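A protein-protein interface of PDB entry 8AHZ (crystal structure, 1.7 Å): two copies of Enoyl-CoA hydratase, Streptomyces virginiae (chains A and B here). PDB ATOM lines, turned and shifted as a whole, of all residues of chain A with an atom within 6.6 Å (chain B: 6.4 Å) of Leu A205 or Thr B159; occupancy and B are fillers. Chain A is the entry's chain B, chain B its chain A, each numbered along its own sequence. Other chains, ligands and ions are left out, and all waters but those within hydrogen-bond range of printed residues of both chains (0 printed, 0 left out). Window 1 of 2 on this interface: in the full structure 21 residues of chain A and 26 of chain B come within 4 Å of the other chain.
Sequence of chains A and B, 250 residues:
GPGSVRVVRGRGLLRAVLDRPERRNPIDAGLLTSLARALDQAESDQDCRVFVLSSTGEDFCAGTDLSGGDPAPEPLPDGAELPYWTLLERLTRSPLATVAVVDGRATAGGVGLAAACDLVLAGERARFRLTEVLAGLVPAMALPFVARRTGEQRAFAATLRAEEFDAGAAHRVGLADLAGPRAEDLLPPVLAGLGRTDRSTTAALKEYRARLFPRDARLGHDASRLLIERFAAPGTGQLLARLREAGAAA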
ATOM      1  N   SER A 200       8.483  16.084  24.397  1.00  0.00           N
ATOM      2  CA  SER A 200       7.532  15.295  23.580  1.00  0.00           C
ATOM      3  C   SER A 200       8.071  13.866  23.421  1.00  0.00           C
ATOM      4  O   SER A 200       7.305  12.869  23.571  1.00  0.00           O
ATOM      5  CB  SER A 200       7.387  15.939  22.240  1.00  0.00           C
ATOM      6  OG  SER A 200       6.460  15.211  21.460  1.00  0.00           O
ATOM      7  N   THR A 201       9.346  13.780  23.074  1.00  0.00           N
ATOM      8  CA  THR A 201      10.011  12.474  22.801  1.00  0.00           C
ATOM      9  C   THR A 201      10.132  11.676  24.104  1.00  0.00           C
ATOM     10  O   THR A 201       9.807  10.462  24.099  1.00  0.00           O
ATOM     11  CB  THR A 201      11.359  12.677  22.104  1.00  0.00           C
ATOM     12  OG1 THR A 201      11.172  13.494  20.934  1.00  0.00           O
ATOM     13  CG2 THR A 201      11.941  11.332  21.718  1.00  0.00           C
ATOM     14  N   THR A 202      10.618  12.282  25.180  1.00  0.00           N
ATOM     15  CA  THR A 202      10.771  11.599  26.489  1.00  0.00           C
ATOM     16  C   THR A 202       9.401  11.094  26.957  1.00  0.00           C
ATOM     17  O   THR A 202       9.262   9.945  27.408  1.00  0.00           O
ATOM     18  CB  THR A 202      11.459  12.522  27.502  1.00  0.00           C
ATOM     19  OG1 THR A 202      12.779  12.823  27.016  1.00  0.00           O
ATOM     20  CG2 THR A 202      11.492  11.887  28.867  1.00  0.00           C
ATOM     21  N   ALA A 203       8.360  11.907  26.835  1.00  0.00           N
ATOM     22  CA  ALA A 203       6.994  11.499  27.212  1.00  0.00           C
ATOM     23  C   ALA A 203       6.541  10.264  26.440  1.00  0.00           C
ATOM     24  O   ALA A 203       5.953   9.360  27.093  1.00  0.00           O
ATOM     25  CB  ALA A 203       6.019  12.642  26.995  1.00  0.00           C
ATOM     26  N   ALA A 204       6.729  10.249  25.129  1.00  0.00           N
ATOM     27  CA  ALA A 204       6.307   9.148  24.240  1.00  0.00           C
ATOM     28  C   ALA A 204       7.103   7.903  24.641  1.00  0.00           C
ATOM     29  O   ALA A 204       6.525   6.811  24.623  1.00  0.00           O
ATOM     30  CB  ALA A 204       6.507   9.513  22.800  1.00  0.00           C
ATOM     31  N   LEU A 205       8.398   8.059  24.932  1.00  0.00           N
ATOM     32  CA  LEU A 205       9.255   6.898  25.309  1.00  0.00           C
ATOM     33  C   LEU A 205       8.720   6.270  26.600  1.00  0.00           C
ATOM     34  O   LEU A 205       8.612   5.046  26.680  1.00  0.00           O
ATOM     35  CB  LEU A 205      10.710   7.360  25.471  1.00  0.00           C
ATOM     36  CG  LEU A 205      11.688   6.270  25.902  1.00  0.00           C
ATOM     37  CD1 LEU A 205      11.799   5.205  24.832  1.00  0.00           C
ATOM     38  CD2 LEU A 205      13.048   6.844  26.212  1.00  0.00           C
ATOM     39  N   LYS A 206       8.393   7.072  27.615  1.00  0.00           N
ATOM     40  CA  LYS A 206       7.959   6.527  28.918  1.00  0.00           C
ATOM     41  C   LYS A 206       6.551   5.941  28.800  1.00  0.00           C
ATOM     42  O   LYS A 206       6.276   4.925  29.451  1.00  0.00           O
ATOM     43  CB  LYS A 206       8.037   7.635  29.965  1.00  0.00           C
ATOM     44  CG  LYS A 206       9.460   8.089  30.217  1.00  0.00           C
ATOM     45  CD  LYS A 206       9.611   9.168  31.252  1.00  0.00           C
ATOM     46  CE  LYS A 206       9.017   8.819  32.591  1.00  0.00           C
ATOM     47  NZ  LYS A 206       9.485   9.777  33.627  1.00  0.00           N
ATOM     48  N   GLU A 207       5.711   6.535  27.966  1.00  0.00           N
ATOM     49  CA  GLU A 207       4.372   5.965  27.705  1.00  0.00           C
ATOM     50  C   GLU A 207       4.545   4.602  27.015  1.00  0.00           C
ATOM     51  O   GLU A 207       3.822   3.643  27.354  1.00  0.00           O
ATOM     52  CB  GLU A 207       3.571   6.929  26.841  1.00  0.00           C
ATOM     53  CG  GLU A 207       2.157   6.457  26.648  1.00  0.00           C
ATOM     54  CD  GLU A 207       1.231   6.642  27.853  1.00  0.00           C
ATOM     55  OE1 GLU A 207       1.690   7.125  28.947  1.00  0.00           O
ATOM     56  OE2 GLU A 207       0.037   6.272  27.693  1.00  0.00           O
ATOM     57  N   TYR A 208       5.497   4.498  26.088  1.00  0.00           N
ATOM     58  CA  TYR A 208       5.736   3.198  25.401  1.00  0.00           C
ATOM     59  C   TYR A 208       6.289   2.148  26.377  1.00  0.00           C
ATOM     60  O   TYR A 208       5.944   0.969  26.286  1.00  0.00           O
ATOM     61  CB  TYR A 208       6.632   3.371  24.181  1.00  0.00           C
ATOM     62  CG  TYR A 208       6.695   2.104  23.364  1.00  0.00           C
ATOM     63  CD1 TYR A 208       5.556   1.537  22.814  1.00  0.00           C
ATOM     64  CD2 TYR A 208       7.894   1.421  23.200  1.00  0.00           C
ATOM     65  CE1 TYR A 208       5.604   0.353  22.093  1.00  0.00           C
ATOM     66  CE2 TYR A 208       7.959   0.264  22.447  1.00  0.00           C
ATOM     67  CZ  TYR A 208       6.814  -0.276  21.883  1.00  0.00           C
ATOM     68  OH  TYR A 208       6.885  -1.454  21.152  1.00  0.00           O
ATOM     69  N   ARG A 209       7.098   2.557  27.356  1.00  0.00           N
ATOM     70  CA  ARG A 209       7.600   1.599  28.370  1.00  0.00           C
ATOM     71  C   ARG A 209       6.412   1.016  29.137  1.00  0.00           C
ATOM     72  O   ARG A 209       6.391  -0.195  29.389  1.00  0.00           O
ATOM     73  CB  ARG A 209       8.586   2.241  29.346  1.00  0.00           C
ATOM     74  CG  ARG A 209       9.254   1.218  30.253  1.00  0.00           C
ATOM     75  CD  ARG A 209      10.298   1.854  31.138  1.00  0.00           C
ATOM     76  NE  ARG A 209      10.860   0.901  32.081  1.00  0.00           N
ATOM     77  CZ  ARG A 209      11.958   1.107  32.795  1.00  0.00           C
ATOM     78  NH1 ARG A 209      12.646   2.232  32.652  1.00  0.00           N
ATOM     79  NH2 ARG A 209      12.375   0.170  33.623  1.00  0.00           N
ATOM     80  N   ALA A 210       5.411   1.834  29.459  1.00  0.00           N
ATOM     81  CA  ALA A 210       4.187   1.359  30.143  1.00  0.00           C
ATOM     82  C   ALA A 210       3.367   0.438  29.233  1.00  0.00           C
ATOM     83  O   ALA A 210       2.748  -0.499  29.748  1.00  0.00           O
ATOM     84  CB  ALA A 210       3.377   2.532  30.632  1.00  0.00           C
ATOM     85  N   LEU B 130      21.098   3.025  19.778  1.00  0.00           N
ATOM     86  CA  LEU B 130      19.763   3.537  19.414  1.00  0.00           C
ATOM     87  C   LEU B 130      19.843   5.060  19.427  1.00  0.00           C
ATOM     88  O   LEU B 130      19.898   5.659  20.523  1.00  0.00           O
ATOM     89  CB  LEU B 130      18.709   2.983  20.367  1.00  0.00           C
ATOM     90  CG  LEU B 130      18.501   1.467  20.310  1.00  0.00           C
ATOM     91  CD1 LEU B 130      17.641   1.004  21.478  1.00  0.00           C
ATOM     92  CD2 LEU B 130      17.874   1.042  19.000  1.00  0.00           C
ATOM     93  N   THR B 131      19.810   5.679  18.256  1.00  0.00           N
ATOM     94  CA  THR B 131      19.980   7.149  18.112  1.00  0.00           C
ATOM     95  C   THR B 131      18.638   7.863  17.959  1.00  0.00           C
ATOM     96  O   THR B 131      18.632   9.126  17.866  1.00  0.00           O
ATOM     97  CB  THR B 131      20.902   7.461  16.938  1.00  0.00           C
ATOM     98  OG1 THR B 131      20.356   6.805  15.794  1.00  0.00           O
ATOM     99  CG2 THR B 131      22.319   7.000  17.207  1.00  0.00           C
ATOM    100  N   GLU B 132      17.543   7.124  17.985  1.00  0.00           N
ATOM    101  CA  GLU B 132      16.192   7.636  17.619  1.00  0.00           C
ATOM    102  C   GLU B 132      15.785   8.879  18.416  1.00  0.00           C
ATOM    103  O   GLU B 132      15.235   9.804  17.787  1.00  0.00           O
ATOM    104  CB  GLU B 132      15.162   6.531  17.800  1.00  0.00           C
ATOM    105  CG  GLU B 132      15.076   5.581  16.603  1.00  0.00           C
ATOM    106  CD  GLU B 132      16.088   4.444  16.502  1.00  0.00           C
ATOM    107  OE1 GLU B 132      17.076   4.417  17.290  1.00  0.00           O
ATOM    108  OE2 GLU B 132      15.853   3.532  15.644  1.00  0.00           O
ATOM    109  N   VAL B 133      16.058   8.947  19.723  1.00  0.00           N
ATOM    110  CA  VAL B 133      15.537  10.091  20.522  1.00  0.00           C
ATOM    111  C   VAL B 133      16.222  11.376  20.051  1.00  0.00           C
ATOM    112  O   VAL B 133      15.631  12.443  20.240  1.00  0.00           O
ATOM    113  CB  VAL B 133      15.696   9.927  22.038  1.00  0.00           C
ATOM    114  CG1 VAL B 133      14.944   8.693  22.503  1.00  0.00           C
ATOM    115  CG2 VAL B 133      17.159   9.939  22.458  1.00  0.00           C
ATOM    116  N   LEU B 134      17.399  11.299  19.424  1.00  0.00           N
ATOM    117  CA  LEU B 134      18.133  12.521  18.986  1.00  0.00           C
ATOM    118  C   LEU B 134      17.403  13.146  17.794  1.00  0.00           C
ATOM    119  O   LEU B 134      17.667  14.314  17.504  1.00  0.00           O
ATOM    120  CB  LEU B 134      19.571  12.171  18.595  1.00  0.00           C
ATOM    121  CG  LEU B 134      20.382  11.501  19.689  1.00  0.00           C
ATOM    122  CD1 LEU B 134      21.711  11.017  19.144  1.00  0.00           C
ATOM    123  CD2 LEU B 134      20.585  12.427  20.870  1.00  0.00           C
ATOM    124  N   LEU B 137      12.411  10.654  17.738  1.00  0.00           N
ATOM    125  CA  LEU B 137      11.722   9.366  17.471  1.00  0.00           C
ATOM    126  C   LEU B 137      11.815   8.432  18.682  1.00  0.00           C
ATOM    127  O   LEU B 137      12.713   8.578  19.537  1.00  0.00           O
ATOM    128  CB  LEU B 137      12.318   8.703  16.229  1.00  0.00           C
ATOM    129  CG  LEU B 137      12.383   9.535  14.955  1.00  0.00           C
ATOM    130  CD1 LEU B 137      13.058   8.731  13.853  1.00  0.00           C
ATOM    131  CD2 LEU B 137      11.005   9.976  14.519  1.00  0.00           C
ATOM    132  N   VAL B 138      10.865   7.510  18.766  1.00  0.00           N
ATOM    133  CA  VAL B 138      10.902   6.363  19.717  1.00  0.00           C
ATOM    134  C   VAL B 138      11.132   5.124  18.879  1.00  0.00           C
ATOM    135  O   VAL B 138      10.346   4.903  17.961  1.00  0.00           O
ATOM    136  CB  VAL B 138       9.607   6.244  20.537  1.00  0.00           C
ATOM    137  CG1 VAL B 138       9.620   4.987  21.399  1.00  0.00           C
ATOM    138  CG2 VAL B 138       9.408   7.477  21.414  1.00  0.00           C
ATOM    139  N   PRO B 139      12.151   4.284  19.193  1.00  0.00           N
ATOM    140  CA  PRO B 139      12.439   3.079  18.414  1.00  0.00           C
ATOM    141  C   PRO B 139      11.486   1.953  18.836  1.00  0.00           C
ATOM    142  O   PRO B 139      11.921   0.925  19.294  1.00  0.00           O
ATOM    143  CB  PRO B 139      13.883   2.741  18.766  1.00  0.00           C
ATOM    144  CG  PRO B 139      14.050   3.270  20.172  1.00  0.00           C
ATOM    145  CD  PRO B 139      13.143   4.485  20.265  1.00  0.00           C
ATOM    146  N   LEU B 143      12.478  -1.928  20.129  1.00  0.00           N
ATOM    147  CA  LEU B 143      12.565  -2.063  21.609  1.00  0.00           C
ATOM    148  C   LEU B 143      12.150  -3.433  22.165  1.00  0.00           C
ATOM    149  O   LEU B 143      12.860  -3.917  23.029  1.00  0.00           O
ATOM    150  CB  LEU B 143      11.846  -0.898  22.294  1.00  0.00           C
ATOM    151  CG  LEU B 143      12.722   0.321  22.568  1.00  0.00           C
ATOM    152  CD1 LEU B 143      11.877   1.551  22.864  1.00  0.00           C
ATOM    153  CD2 LEU B 143      13.691   0.045  23.705  1.00  0.00           C
ATOM    154  N   VAL B 146      15.054  -5.722  21.680  1.00  0.00           N
ATOM    155  CA  VAL B 146      16.197  -5.323  22.542  1.00  0.00           C
ATOM    156  C   VAL B 146      15.866  -5.698  24.005  1.00  0.00           C
ATOM    157  O   VAL B 146      16.711  -6.358  24.679  1.00  0.00           O
ATOM    158  CB  VAL B 146      16.511  -3.830  22.380  1.00  0.00           C
ATOM    159  CG1 VAL B 146      17.568  -3.393  23.384  1.00  0.00           C
ATOM    160  CG2 VAL B 146      16.945  -3.511  20.955  1.00  0.00           C
ATOM    161  N   ARG B 154      17.553  -1.407  31.093  1.00  0.00           N
ATOM    162  CA  ARG B 154      18.743  -1.046  30.264  1.00  0.00           C
ATOM    163  C   ARG B 154      18.278  -0.686  28.840  1.00  0.00           C
ATOM    164  O   ARG B 154      18.885   0.243  28.250  1.00  0.00           O
ATOM    165  CB  ARG B 154      19.823  -2.136  30.245  1.00  0.00           C
ATOM    166  CG  ARG B 154      21.153  -1.688  29.640  1.00  0.00           C
ATOM    167  CD  ARG B 154      21.649  -0.350  30.163  1.00  0.00           C
ATOM    168  NE  ARG B 154      23.071  -0.082  29.967  1.00  0.00           N
ATOM    169  CZ  ARG B 154      24.060  -0.646  30.641  1.00  0.00           C
ATOM    170  NH1 ARG B 154      23.817  -1.524  31.600  1.00  0.00           N
ATOM    171  NH2 ARG B 154      25.313  -0.319  30.363  1.00  0.00           N
ATOM    172  N   ALA B 155      17.260  -1.355  28.285  1.00  0.00           N
ATOM    173  CA  ALA B 155      16.749  -1.020  26.922  1.00  0.00           C
ATOM    174  C   ALA B 155      16.219   0.423  26.893  1.00  0.00           C
ATOM    175  O   ALA B 155      16.610   1.193  26.005  1.00  0.00           O
ATOM    176  CB  ALA B 155      15.683  -1.988  26.475  1.00  0.00           C
ATOM    177  N   PHE B 156      15.402   0.805  27.871  1.00  0.00           N
ATOM    178  CA  PHE B 156      14.762   2.143  27.885  1.00  0.00           C
ATOM    179  C   PHE B 156      15.777   3.213  28.302  1.00  0.00           C
ATOM    180  O   PHE B 156      15.762   4.310  27.704  1.00  0.00           O
ATOM    181  CB  PHE B 156      13.488   2.084  28.723  1.00  0.00           C
ATOM    182  CG  PHE B 156      12.333   1.557  27.910  1.00  0.00           C
ATOM    183  CD1 PHE B 156      12.115   0.192  27.778  1.00  0.00           C
ATOM    184  CD2 PHE B 156      11.507   2.425  27.201  1.00  0.00           C
ATOM    185  CE1 PHE B 156      11.087  -0.293  26.979  1.00  0.00           C
ATOM    186  CE2 PHE B 156      10.488   1.939  26.387  1.00  0.00           C
ATOM    187  CZ  PHE B 156      10.272   0.581  26.292  1.00  0.00           C
ATOM    188  N   ALA B 157      16.670   2.927  29.246  1.00  0.00           N
ATOM    189  CA  ALA B 157      17.703   3.912  29.661  1.00  0.00           C
ATOM    190  C   ALA B 157      18.697   4.143  28.509  1.00  0.00           C
ATOM    191  O   ALA B 157      19.079   5.311  28.261  1.00  0.00           O
ATOM    192  CB  ALA B 157      18.412   3.483  30.943  1.00  0.00           C
ATOM    193  N   ALA B 158      19.088   3.076  27.791  1.00  0.00           N
ATOM    194  CA  ALA B 158      20.009   3.162  26.639  1.00  0.00           C
ATOM    195  C   ALA B 158      19.347   3.989  25.529  1.00  0.00           C
ATOM    196  O   ALA B 158      20.043   4.752  24.829  1.00  0.00           O
ATOM    197  CB  ALA B 158      20.338   1.798  26.142  1.00  0.00           C
ATOM    198  N   THR B 159      18.027   3.898  25.424  1.00  0.00           N
ATOM    199  CA  THR B 159      17.268   4.662  24.405  1.00  0.00           C
ATOM    200  C   THR B 159      17.251   6.132  24.816  1.00  0.00           C
ATOM    201  O   THR B 159      17.586   7.012  23.979  1.00  0.00           O
ATOM    202  CB  THR B 159      15.855   4.109  24.217  1.00  0.00           C
ATOM    203  OG1 THR B 159      15.956   2.760  23.739  1.00  0.00           O
ATOM    204  CG2 THR B 159      15.053   4.924  23.230  1.00  0.00           C
ATOM    205  N   LEU B 160      16.908   6.413  26.070  1.00  0.00           N
ATOM    206  CA  LEU B 160      16.816   7.809  26.592  1.00  0.00           C
ATOM    207  C   LEU B 160      18.180   8.507  26.472  1.00  0.00           C
ATOM    208  O   LEU B 160      18.226   9.725  26.146  1.00  0.00           O
ATOM    209  CB  LEU B 160      16.339   7.770  28.038  1.00  0.00           C
ATOM    210  CG  LEU B 160      16.209   9.116  28.757  1.00  0.00           C
ATOM    211  CD1 LEU B 160      15.205  10.016  28.059  1.00  0.00           C
ATOM    212  CD2 LEU B 160      15.804   8.902  30.205  1.00  0.00           C
ATOM    213  N   ARG B 161      19.278   7.780  26.685  1.00  0.00           N
ATOM    214  CA  ARG B 161      20.660   8.351  26.681  1.00  0.00           C
ATOM    215  C   ARG B 161      21.363   8.194  25.317  1.00  0.00           C
ATOM    216  O   ARG B 161      22.509   8.663  25.201  1.00  0.00           O
ATOM    217  CB  ARG B 161      21.496   7.664  27.765  1.00  0.00           C
ATOM    218  CG  ARG B 161      21.019   7.909  29.192  1.00  0.00           C
ATOM    219  CD  ARG B 161      21.853   7.132  30.188  1.00  0.00           C
ATOM    220  NE  ARG B 161      23.230   7.596  30.179  1.00  0.00           N
ATOM    221  CZ  ARG B 161      24.300   6.812  30.195  1.00  0.00           C
ATOM    222  NH1 ARG B 161      24.194   5.489  30.194  1.00  0.00           N
ATOM    223  NH2 ARG B 161      25.494   7.371  30.197  1.00  0.00           N
ATOM    224  N   ALA B 162      20.757   7.525  24.325  1.00  0.00           N
ATOM    225  CA  ALA B 162      21.425   7.121  23.059  1.00  0.00           C
ATOM    226  C   ALA B 162      22.781   6.495  23.382  1.00  0.00           C
ATOM    227  O   ALA B 162      23.814   6.922  22.808  1.00  0.00           O
ATOM    228  CB  ALA B 162      21.555   8.302  22.122  1.00  0.00           C
ATOM    229  N   GLU B 163      22.786   5.562  24.328  1.00  0.00           N
ATOM    230  CA  GLU B 163      24.010   4.917  24.856  1.00  0.00           C
ATOM    231  C   GLU B 163      24.643   4.064  23.754  1.00  0.00           C
ATOM    232  O   GLU B 163      23.923   3.303  23.091  1.00  0.00           O
ATOM    233  CB  GLU B 163      23.661   4.030  26.055  1.00  0.00           C
ATOM    234  CG  GLU B 163      24.830   3.294  26.674  1.00  0.00           C
ATOM    235  CD  GLU B 163      24.469   2.467  27.913  1.00  0.00           C
ATOM    236  OE1 GLU B 163      23.260   2.413  28.263  1.00  0.00           O
ATOM    237  OE2 GLU B 163      25.412   1.891  28.543  1.00  0.00           O
ATOM    238  N   LEU B 226       3.272   4.189  16.505  1.00  0.00           N
ATOM    239  CA  LEU B 226       4.046   5.199  17.279  1.00  0.00           C
ATOM    240  C   LEU B 226       5.178   5.785  16.419  1.00  0.00           C
ATOM    241  O   LEU B 226       5.408   6.993  16.503  1.00  0.00           O
ATOM    242  CB  LEU B 226       4.648   4.564  18.536  1.00  0.00           C
ATOM    243  CG  LEU B 226       5.408   5.525  19.444  1.00  0.00           C
ATOM    244  CD1 LEU B 226       4.591   6.783  19.753  1.00  0.00           C
ATOM    245  CD2 LEU B 226       5.790   4.820  20.732  1.00  0.00           C
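Among the printed residues, pairs that only touch across the chains: Arg A209 with Phe B156 (3.5 Å), Thr A201 with Leu B137 (3.6 Å), Leu A205 with Thr B159 (3.6 Å), Leu A205 with Phe B156 (3.6 Å), Leu A205 with Val B138 (3.7 Å), Ala A204 with Val B138 (3.8 Å), Tyr A208 with Leu B226 (3.8 Å), Thr A202 with Leu B160 (3.9 Å), Leu A205 with Leu B160 (3.9 Å), Thr A201 with Val B133 (3.99 Å), Tyr A208 with Phe B156 (3.99 Å) and Tyr A208 with Leu B143 (3.999 Å).
Of the 21 printed residues of chain B, 8 touch a printed residue of chain A.
Printed residues of chain B that touch a printed residue of chain A: Val B133, Leu B137, Val B138, Leu B143, Phe B156, Thr B159, Leu B160 and Leu B226.
Hydrophobic or aromatic side chains of chain B within 4 Å of the printed part of chain A: Val B138, Leu B143, Phe B156, Leu B160 and Leu B226.
Of the 11 printed residues of chain A, 6 touch a printed residue of chain B.
Printed residues of chain A that touch a printed residue of chain B: Thr A201, Thr A202, Ala A204, Leu A205, Tyr A208 and Arg A209.
Hydrophobic or aromatic side chains of chain A that line the printed part of chain B: Ala A204, Leu A205 and Tyr A208.
Among the printed residues, 12 pairs touch across the chains.
Among the printed residues, no Asp or Glu carboxylate lies within 4 Å of a Lys or Arg side-chain nitrogen of the other chain.
Of chain B, only Val B138 (3.7 Å), Phe B156 (3.6 Å), Thr B159 (3.6 Å) and Leu B160 (3.9 Å) come within 4 Å of Leu A205.
Thr B159 touches just one residue of chain A: Leu A205 (3.6 Å).
Of the printed residues of chain B, Thr A201 touches Val B133 and Leu B137.
Of the printed residues of chain A, Leu B143 touches Tyr A208.
Ser A200 touches none of the printed residues of chain B.
The nearest residue of chain B that does not touch Leu A205 is Leu B143 (4.2 Å).
The nearest printed residue of chain A that does not touch Thr B159 is Thr A201 (7.3 Å).
No position is printed for both chains.
The backbone carbonyl oxygen (O) of Glu B132 sits at hydrogen-bond distance from the backbone NH (N) of Leu B137 (2.9 Å).
O of Ala B155 lies within hydrogen-bond range of OG1 of Thr B159 (2.8 Å).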
